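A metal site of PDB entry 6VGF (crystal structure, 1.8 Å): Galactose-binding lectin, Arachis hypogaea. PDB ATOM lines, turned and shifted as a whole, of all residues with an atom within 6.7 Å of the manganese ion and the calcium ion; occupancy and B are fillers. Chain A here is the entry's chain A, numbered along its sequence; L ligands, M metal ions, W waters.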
ATOM      1  N   ASP A  83     -17.418  -2.745   9.506  1.00  0.00           N
ATOM      2  CA  ASP A  83     -16.647  -2.344  10.692  1.00  0.00           C
ATOM      3  C   ASP A  83     -15.361  -1.567  10.449  1.00  0.00           C
ATOM      4  O   ASP A  83     -14.802  -1.007  11.397  1.00  0.00           O
ATOM      5  CB  ASP A  83     -16.321  -3.560  11.537  1.00  0.00           C
ATOM      6  CG  ASP A  83     -17.480  -3.913  12.434  1.00  0.00           C
ATOM      7  OD1 ASP A  83     -17.558  -3.339  13.550  1.00  0.00           O
ATOM      8  OD2 ASP A  83     -18.356  -4.725  11.997  1.00  0.00           O
ATOM      9  N   GLY A 103     -17.047  -8.653  12.428  1.00  0.00           N
ATOM     10  CA  GLY A 103     -17.329  -7.479  13.252  1.00  0.00           C
ATOM     11  C   GLY A 103     -16.105  -6.658  13.653  1.00  0.00           C
ATOM     12  O   GLY A 103     -15.297  -6.281  12.794  1.00  0.00           O
ATOM     13  N   GLY A 104     -15.970  -6.409  14.961  1.00  0.00           N
ATOM     14  CA  GLY A 104     -14.896  -5.625  15.564  1.00  0.00           C
ATOM     15  C   GLY A 104     -13.516  -6.267  15.517  1.00  0.00           C
ATOM     16  O   GLY A 104     -12.528  -5.595  15.818  1.00  0.00           O
ATOM     17  N   THR A 105     -13.452  -7.580  15.175  1.00  0.00           N
ATOM     18  CA  THR A 105     -12.191  -8.322  15.079  1.00  0.00           C
ATOM     19  C   THR A 105     -11.410  -7.898  13.831  1.00  0.00           C
ATOM     20  O   THR A 105     -10.249  -8.282  13.689  1.00  0.00           O
ATOM     21  CB  THR A 105     -12.434  -9.865  15.089  1.00  0.00           C
ATOM     22  OG1 THR A 105     -12.925 -10.320  13.818  1.00  0.00           O
ATOM     23  CG2 THR A 105     -13.325 -10.317  16.230  1.00  0.00           C
ATOM     24  N   LEU A 106     -12.101  -7.228  12.878  1.00  0.00           N
ATOM     25  CA  LEU A 106     -11.597  -6.719  11.595  1.00  0.00           C
ATOM     26  C   LEU A 106     -10.981  -7.858  10.738  1.00  0.00           C
ATOM     27  O   LEU A 106     -10.217  -7.597   9.804  1.00  0.00           O
ATOM     28  CB  LEU A 106     -10.565  -5.567  11.818  1.00  0.00           C
ATOM     29  CG  LEU A 106     -11.097  -4.320  12.519  1.00  0.00           C
ATOM     30  CD1 LEU A 106      -9.957  -3.314  12.751  1.00  0.00           C
ATOM     31  CD2 LEU A 106     -12.262  -3.667  11.769  1.00  0.00           C
ATOM     32  N   GLU A 121      -5.382   0.230  11.514  1.00  0.00           N
ATOM     33  CA  GLU A 121      -6.838   0.104  11.323  1.00  0.00           C
ATOM     34  C   GLU A 121      -7.506   1.445  11.056  1.00  0.00           C
ATOM     35  O   GLU A 121      -7.091   2.481  11.583  1.00  0.00           O
ATOM     36  CB  GLU A 121      -7.505  -0.571  12.532  1.00  0.00           C
ATOM     37  CG  GLU A 121      -7.244   0.167  13.826  1.00  0.00           C
ATOM     38  CD  GLU A 121      -8.175  -0.270  14.926  1.00  0.00           C
ATOM     39  OE1 GLU A 121      -8.105  -1.462  15.296  1.00  0.00           O
ATOM     40  OE2 GLU A 121      -8.970   0.559  15.395  1.00  0.00           O
ATOM     41  N   ASP A 123     -11.034   2.241  11.614  1.00  0.00           N
ATOM     42  CA  ASP A 123     -12.155   1.705  12.372  1.00  0.00           C
ATOM     43  C   ASP A 123     -13.352   2.640  12.405  1.00  0.00           C
ATOM     44  O   ASP A 123     -13.236   3.773  12.869  1.00  0.00           O
ATOM     45  CB  ASP A 123     -11.641   1.419  13.790  1.00  0.00           C
ATOM     46  CG  ASP A 123     -12.531   0.496  14.590  1.00  0.00           C
ATOM     47  OD1 ASP A 123     -13.669   0.221  14.134  1.00  0.00           O
ATOM     48  OD2 ASP A 123     -12.069  -0.009  15.623  1.00  0.00           O
ATOM     49  N   THR A 124     -14.520   2.136  11.922  1.00  0.00           N
ATOM     50  CA  THR A 124     -15.730   2.950  11.783  1.00  0.00           C
ATOM     51  C   THR A 124     -16.862   2.572  12.763  1.00  0.00           C
ATOM     52  O   THR A 124     -17.988   3.073  12.604  1.00  0.00           O
ATOM     53  CB  THR A 124     -16.240   2.892  10.337  1.00  0.00           C
ATOM     54  OG1 THR A 124     -16.804   1.615  10.056  1.00  0.00           O
ATOM     55  CG2 THR A 124     -15.151   3.205   9.333  1.00  0.00           C
ATOM     56  N   TYR A 125     -16.570   1.767  13.791  1.00  0.00           N
ATOM     57  CA  TYR A 125     -17.549   1.362  14.814  1.00  0.00           C
ATOM     58  C   TYR A 125     -16.859   1.173  16.169  1.00  0.00           C
ATOM     59  O   TYR A 125     -15.852   0.473  16.258  1.00  0.00           O
ATOM     60  CB  TYR A 125     -18.308   0.077  14.408  1.00  0.00           C
ATOM     61  CG  TYR A 125     -19.369  -0.271  15.435  1.00  0.00           C
ATOM     62  CD1 TYR A 125     -19.071  -1.078  16.528  1.00  0.00           C
ATOM     63  CD2 TYR A 125     -20.638   0.286  15.364  1.00  0.00           C
ATOM     64  CE1 TYR A 125     -20.005  -1.320  17.532  1.00  0.00           C
ATOM     65  CE2 TYR A 125     -21.603   0.017  16.338  1.00  0.00           C
ATOM     66  CZ  TYR A 125     -21.278  -0.766  17.430  1.00  0.00           C
ATOM     67  OH  TYR A 125     -22.226  -1.035  18.376  1.00  0.00           O
ATOM     68  N   SER A 126     -17.441   1.758  17.237  1.00  0.00           N
ATOM     69  CA  SER A 126     -16.886   1.703  18.591  1.00  0.00           C
ATOM     70  C   SER A 126     -17.292   0.428  19.334  1.00  0.00           C
ATOM     71  O   SER A 126     -18.429   0.309  19.789  1.00  0.00           O
ATOM     72  CB  SER A 126     -17.304   2.943  19.387  1.00  0.00           C
ATOM     73  OG  SER A 126     -16.601   2.992  20.618  1.00  0.00           O
ATOM     74  N   ASN A 127     -16.345  -0.536  19.441  1.00  0.00           N
ATOM     75  CA  ASN A 127     -16.488  -1.795  20.163  1.00  0.00           C
ATOM     76  C   ASN A 127     -15.950  -1.645  21.583  1.00  0.00           C
ATOM     77  O   ASN A 127     -14.736  -1.666  21.795  1.00  0.00           O
ATOM     78  CB  ASN A 127     -15.756  -2.935  19.441  1.00  0.00           C
ATOM     79  CG  ASN A 127     -16.295  -3.214  18.070  1.00  0.00           C
ATOM     80  OD1 ASN A 127     -16.039  -2.471  17.118  1.00  0.00           O
ATOM     81  ND2 ASN A 127     -17.070  -4.267  17.942  1.00  0.00           N
ATOM     82  N   TYR A 130     -13.368  -4.027  22.960  1.00  0.00           N
ATOM     83  CA  TYR A 130     -11.970  -3.866  22.520  1.00  0.00           C
ATOM     84  C   TYR A 130     -11.417  -2.480  22.920  1.00  0.00           C
ATOM     85  O   TYR A 130     -10.373  -2.057  22.424  1.00  0.00           O
ATOM     86  CB  TYR A 130     -11.843  -4.100  21.005  1.00  0.00           C
ATOM     87  CG  TYR A 130     -12.434  -5.431  20.554  1.00  0.00           C
ATOM     88  CD1 TYR A 130     -12.123  -6.610  21.223  1.00  0.00           C
ATOM     89  CD2 TYR A 130     -13.244  -5.504  19.435  1.00  0.00           C
ATOM     90  CE1 TYR A 130     -12.679  -7.823  20.836  1.00  0.00           C
ATOM     91  CE2 TYR A 130     -13.818  -6.713  19.043  1.00  0.00           C
ATOM     92  CZ  TYR A 130     -13.520  -7.871  19.746  1.00  0.00           C
ATOM     93  OH  TYR A 130     -14.045  -9.066  19.340  1.00  0.00           O
ATOM     94  N   ASN A 131     -12.130  -1.798  23.841  1.00  0.00           N
ATOM     95  CA  ASN A 131     -11.816  -0.475  24.390  1.00  0.00           C
ATOM     96  C   ASN A 131     -11.608   0.573  23.290  1.00  0.00           C
ATOM     97  O   ASN A 131     -10.712   1.406  23.383  1.00  0.00           O
ATOM     98  CB  ASN A 131     -10.595  -0.550  25.344  1.00  0.00           C
ATOM     99  CG  ASN A 131     -10.875  -1.317  26.608  1.00  0.00           C
ATOM    100  OD1 ASN A 131     -11.793  -1.004  27.368  1.00  0.00           O
ATOM    101  ND2 ASN A 131     -10.072  -2.354  26.851  1.00  0.00           N
ATOM    102  N   ASP A 132     -12.452   0.513  22.244  1.00  0.00           N
ATOM    103  CA  ASP A 132     -12.403   1.469  21.137  1.00  0.00           C
ATOM    104  C   ASP A 132     -12.716   2.877  21.612  1.00  0.00           C
ATOM    105  O   ASP A 132     -13.611   3.019  22.455  1.00  0.00           O
ATOM    106  CB  ASP A 132     -13.440   1.109  20.052  1.00  0.00           C
ATOM    107  CG  ASP A 132     -12.938   0.213  18.945  1.00  0.00           C
ATOM    108  OD1 ASP A 132     -11.708   0.138  18.747  1.00  0.00           O
ATOM    109  OD2 ASP A 132     -13.779  -0.371  18.235  1.00  0.00           O
ATOM    110  N   PRO A 133     -12.100   3.931  21.047  1.00  0.00           N
ATOM    111  CA  PRO A 133     -12.510   5.300  21.442  1.00  0.00           C
ATOM    112  C   PRO A 133     -13.960   5.578  20.975  1.00  0.00           C
ATOM    113  O   PRO A 133     -14.484   4.791  20.177  1.00  0.00           O
ATOM    114  CB  PRO A 133     -11.465   6.199  20.767  1.00  0.00           C
ATOM    115  CG  PRO A 133     -10.925   5.394  19.637  1.00  0.00           C
ATOM    116  CD  PRO A 133     -11.028   3.949  20.023  1.00  0.00           C
ATOM    117  N   HIS A 137     -11.777   6.172  14.125  1.00  0.00           N
ATOM    118  CA  HIS A 137     -10.381   6.363  14.467  1.00  0.00           C
ATOM    119  C   HIS A 137      -9.423   5.535  13.611  1.00  0.00           C
ATOM    120  O   HIS A 137      -9.780   4.483  13.087  1.00  0.00           O
ATOM    121  CB  HIS A 137     -10.144   6.000  15.949  1.00  0.00           C
ATOM    122  CG  HIS A 137     -10.636   4.621  16.306  1.00  0.00           C
ATOM    123  ND1 HIS A 137     -12.003   4.354  16.494  1.00  0.00           N
ATOM    124  CD2 HIS A 137      -9.943   3.482  16.501  1.00  0.00           C
ATOM    125  CE1 HIS A 137     -12.071   3.078  16.817  1.00  0.00           C
ATOM    126  NE2 HIS A 137     -10.851   2.513  16.820  1.00  0.00           N
ATOM    127  N   VAL A 138      -8.188   6.003  13.573  1.00  0.00           N
ATOM    128  CA  VAL A 138      -7.069   5.302  12.986  1.00  0.00           C
ATOM    129  C   VAL A 138      -6.307   4.747  14.175  1.00  0.00           C
ATOM    130  O   VAL A 138      -6.111   5.463  15.172  1.00  0.00           O
ATOM    131  CB  VAL A 138      -6.201   6.149  12.012  1.00  0.00           C
ATOM    132  CG1 VAL A 138      -5.045   5.325  11.449  1.00  0.00           C
ATOM    133  CG2 VAL A 138      -7.035   6.713  10.872  1.00  0.00           C
ATOM    134  N   GLY A 139      -5.988   3.466  14.140  1.00  0.00           N
ATOM    135  CA  GLY A 139      -5.298   2.855  15.256  1.00  0.00           C
ATOM    136  C   GLY A 139      -4.050   2.115  14.845  1.00  0.00           C
ATOM    137  O   GLY A 139      -3.941   1.717  13.696  1.00  0.00           O
ATOM    138  N   ASP A 141      -2.059  -1.208  15.831  1.00  0.00           N
ATOM    139  CA  ASP A 141      -2.391  -2.476  16.492  1.00  0.00           C
ATOM    140  C   ASP A 141      -1.223  -3.425  16.571  1.00  0.00           C
ATOM    141  O   ASP A 141      -0.574  -3.679  15.575  1.00  0.00           O
ATOM    142  CB  ASP A 141      -3.549  -3.162  15.760  1.00  0.00           C
ATOM    143  CG  ASP A 141      -4.866  -2.416  15.784  1.00  0.00           C
ATOM    144  OD1 ASP A 141      -4.994  -1.434  16.551  1.00  0.00           O
ATOM    145  OD2 ASP A 141      -5.800  -2.855  15.087  1.00  0.00           O
ATOM    146  N   VAL A 145      -6.785  -5.955  18.535  1.00  0.00           N
ATOM    147  CA  VAL A 145      -7.649  -4.905  18.019  1.00  0.00           C
ATOM    148  C   VAL A 145      -7.960  -3.918  19.180  1.00  0.00           C
ATOM    149  O   VAL A 145      -8.683  -2.940  18.984  1.00  0.00           O
ATOM    150  CB  VAL A 145      -8.935  -5.367  17.267  1.00  0.00           C
ATOM    151  CG1 VAL A 145      -8.579  -5.980  15.906  1.00  0.00           C
ATOM    152  CG2 VAL A 145      -9.751  -6.336  18.110  1.00  0.00           C
ATOM    153  N   ASP A 146      -7.382  -4.145  20.378  1.00  0.00           N
ATOM    154  CA  ASP A 146      -7.371  -3.158  21.470  1.00  0.00           C
ATOM    155  C   ASP A 146      -6.074  -2.382  21.177  1.00  0.00           C
ATOM    156  O   ASP A 146      -4.993  -2.808  21.572  1.00  0.00           O
ATOM    157  CB  ASP A 146      -7.451  -3.814  22.858  1.00  0.00           C
ATOM    158  CG  ASP A 146      -7.551  -2.841  24.048  1.00  0.00           C
ATOM    159  OD1 ASP A 146      -7.167  -1.658  23.903  1.00  0.00           O
ATOM    160  OD2 ASP A 146      -7.990  -3.265  25.137  1.00  0.00           O
ATOM    161  N   SER A 147      -6.196  -1.322  20.381  1.00  0.00           N
ATOM    162  CA  SER A 147      -5.069  -0.560  19.845  1.00  0.00           C
ATOM    163  C   SER A 147      -4.064  -0.072  20.885  1.00  0.00           C
ATOM    164  O   SER A 147      -4.437   0.393  21.974  1.00  0.00           O
ATOM    165  CB  SER A 147      -5.555   0.647  19.047  1.00  0.00           C
ATOM    166  OG  SER A 147      -6.385   0.312  17.961  1.00  0.00           O
ATOM    167  N   THR A 150      -4.503   5.277  19.269  1.00  0.00           N
ATOM    168  CA  THR A 150      -5.499   5.715  18.285  1.00  0.00           C
ATOM    169  C   THR A 150      -5.444   7.225  18.135  1.00  0.00           C
ATOM    170  O   THR A 150      -4.914   7.925  18.995  1.00  0.00           O
ATOM    171  CB  THR A 150      -6.961   5.291  18.626  1.00  0.00           C
ATOM    172  OG1 THR A 150      -7.441   5.976  19.773  1.00  0.00           O
ATOM    173  CG2 THR A 150      -7.152   3.805  18.747  1.00  0.00           C
HETATM  174  C1  LIG L   1     -22.050  -5.506  16.552  1.00  0.00           C
HETATM  175  S1  LIG L   1     -22.983  -7.013  16.893  1.00  0.00           S
HETATM  176  C2  LIG L   1     -20.586  -5.824  16.261  1.00  0.00           C
HETATM  177  O1  LIG L   1     -19.968  -6.409  17.401  1.00  0.00           O
HETATM  178  C3  LIG L   1     -19.821  -4.561  15.874  1.00  0.00           C
HETATM  179  O2  LIG L   1     -18.493  -4.892  15.521  1.00  0.00           O
HETATM  180  C4  LIG L   1     -20.550  -3.825  14.744  1.00  0.00           C
HETATM  181  O3  LIG L   1     -20.492  -4.569  13.527  1.00  0.00           O
HETATM  182  C5  LIG L   1     -21.988  -3.565  15.177  1.00  0.00           C
HETATM  183  O4  LIG L   1     -22.641  -4.815  15.456  1.00  0.00           O
HETATM  184  C6  LIG L   1     -22.830  -2.841  14.155  1.00  0.00           C
HETATM  185  O5  LIG L   1     -23.986  -2.261  14.773  1.00  0.00           O
HETATM  186  C7  LIG L   1     -24.352  -6.347  17.892  1.00  0.00           C
HETATM  187  C8  LIG L   1     -25.584  -7.252  17.850  1.00  0.00           C
HETATM  188  O6  LIG L   1     -25.994  -7.461  16.496  1.00  0.00           O
HETATM  189  C9  LIG L   1     -26.693  -6.599  18.667  1.00  0.00           C
HETATM  190  O7  LIG L   1     -27.862  -7.406  18.687  1.00  0.00           O
HETATM  191  C10 LIG L   1     -26.224  -6.300  20.094  1.00  0.00           C
HETATM  192  O8  LIG L   1     -27.213  -5.518  20.758  1.00  0.00           O
HETATM  193  C11 LIG L   1     -24.893  -5.535  20.101  1.00  0.00           C
HETATM  194  O9  LIG L   1     -23.927  -6.165  19.243  1.00  0.00           O
HETATM  195  C12 LIG L   1     -24.197  -5.581  21.445  1.00  0.00           C
HETATM  196  C13 LIG L   1     -10.288 -16.059  38.435  1.00  0.00           C
HETATM  197 MN    MN M   1     -10.514   0.483  16.944  1.00  0.00          MN
HETATM  198 CA    CA M   2     -14.317  -1.048  16.091  1.00  0.00          CA
HETATM  199  O   HOH W   1      -9.038   1.006  18.369  1.00  0.00           O
HETATM  200  O   HOH W   2     -12.768  -2.937  16.381  1.00  0.00           O
HETATM  201  O   HOH W   3     -15.061  -2.140  14.253  1.00  0.00           O
HETATM  202  O   HOH W   4     -10.088  -1.934  16.992  1.00  0.00           O
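The manganese ion is bound by a ring nitrogen (NE2) of His 137 (2.1 Å), the side-chain carboxylate (OD2) of Asp 123 (2.1 Å), water W1 (2.1 Å), the side-chain carboxylate (OE2) of Glu 121 (2.2 Å), the side-chain carboxylate (OD1) of Asp 132 (2.2 Å) and water W4 (2.5 Å).
The calcium ion is bound by the backbone carbonyl oxygen (O) of Tyr 125 (2.2 Å), water W3 (2.3 Å), the side-chain carboxylate (OD2) of Asp 132 (2.3 Å), the side-chain carboxylate (OD1) of Asp 123 (2.4 Å), the side-chain amide oxygen (OD1) of Asn 127 (2.5 Å), water W2 (2.5 Å) and the side-chain carboxylate (OD2) of Asp 123 (2.5 Å).
Of the 23 residues printed, 4 come within 4 Å of the manganese ion. The nearest printed residue that does not touch the manganese ion is Ser 147 (4.3 Å).
Water W4 bridges O of Val 145 and OE1 of Glu 121.
Four residues have an atom within 4 Å of the calcium ion: Asp 123, Tyr 125, Asn 127 and Asp 132. The nearest printed residue that does not touch the calcium ion is Ser 126 (4.4 Å).
The side-chain carboxylate (OE1) of Glu 121 sits close to the side-chain carboxylate (OD2) of Asp 141 (2.7 Å). The backbone carbonyl oxygen of Glu 121 is in hydrogen-bond range of the backbone NH of Gly 139, 3.0 Å away.
The side-chain carboxylate (OD2) of Asp 83 sits at hydrogen-bond distance from an oxygen (O3) of the ligand (2.6 Å). The side-chain amide nitrogen (ND2) of Asn 127 sits at hydrogen-bond distance from an oxygen (O2) of the ligand, 2.9 Å away. The backbone NH (N) of Gly 104 is in hydrogen-bond range of an oxygen (O2) of the ligand (3.0 Å).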
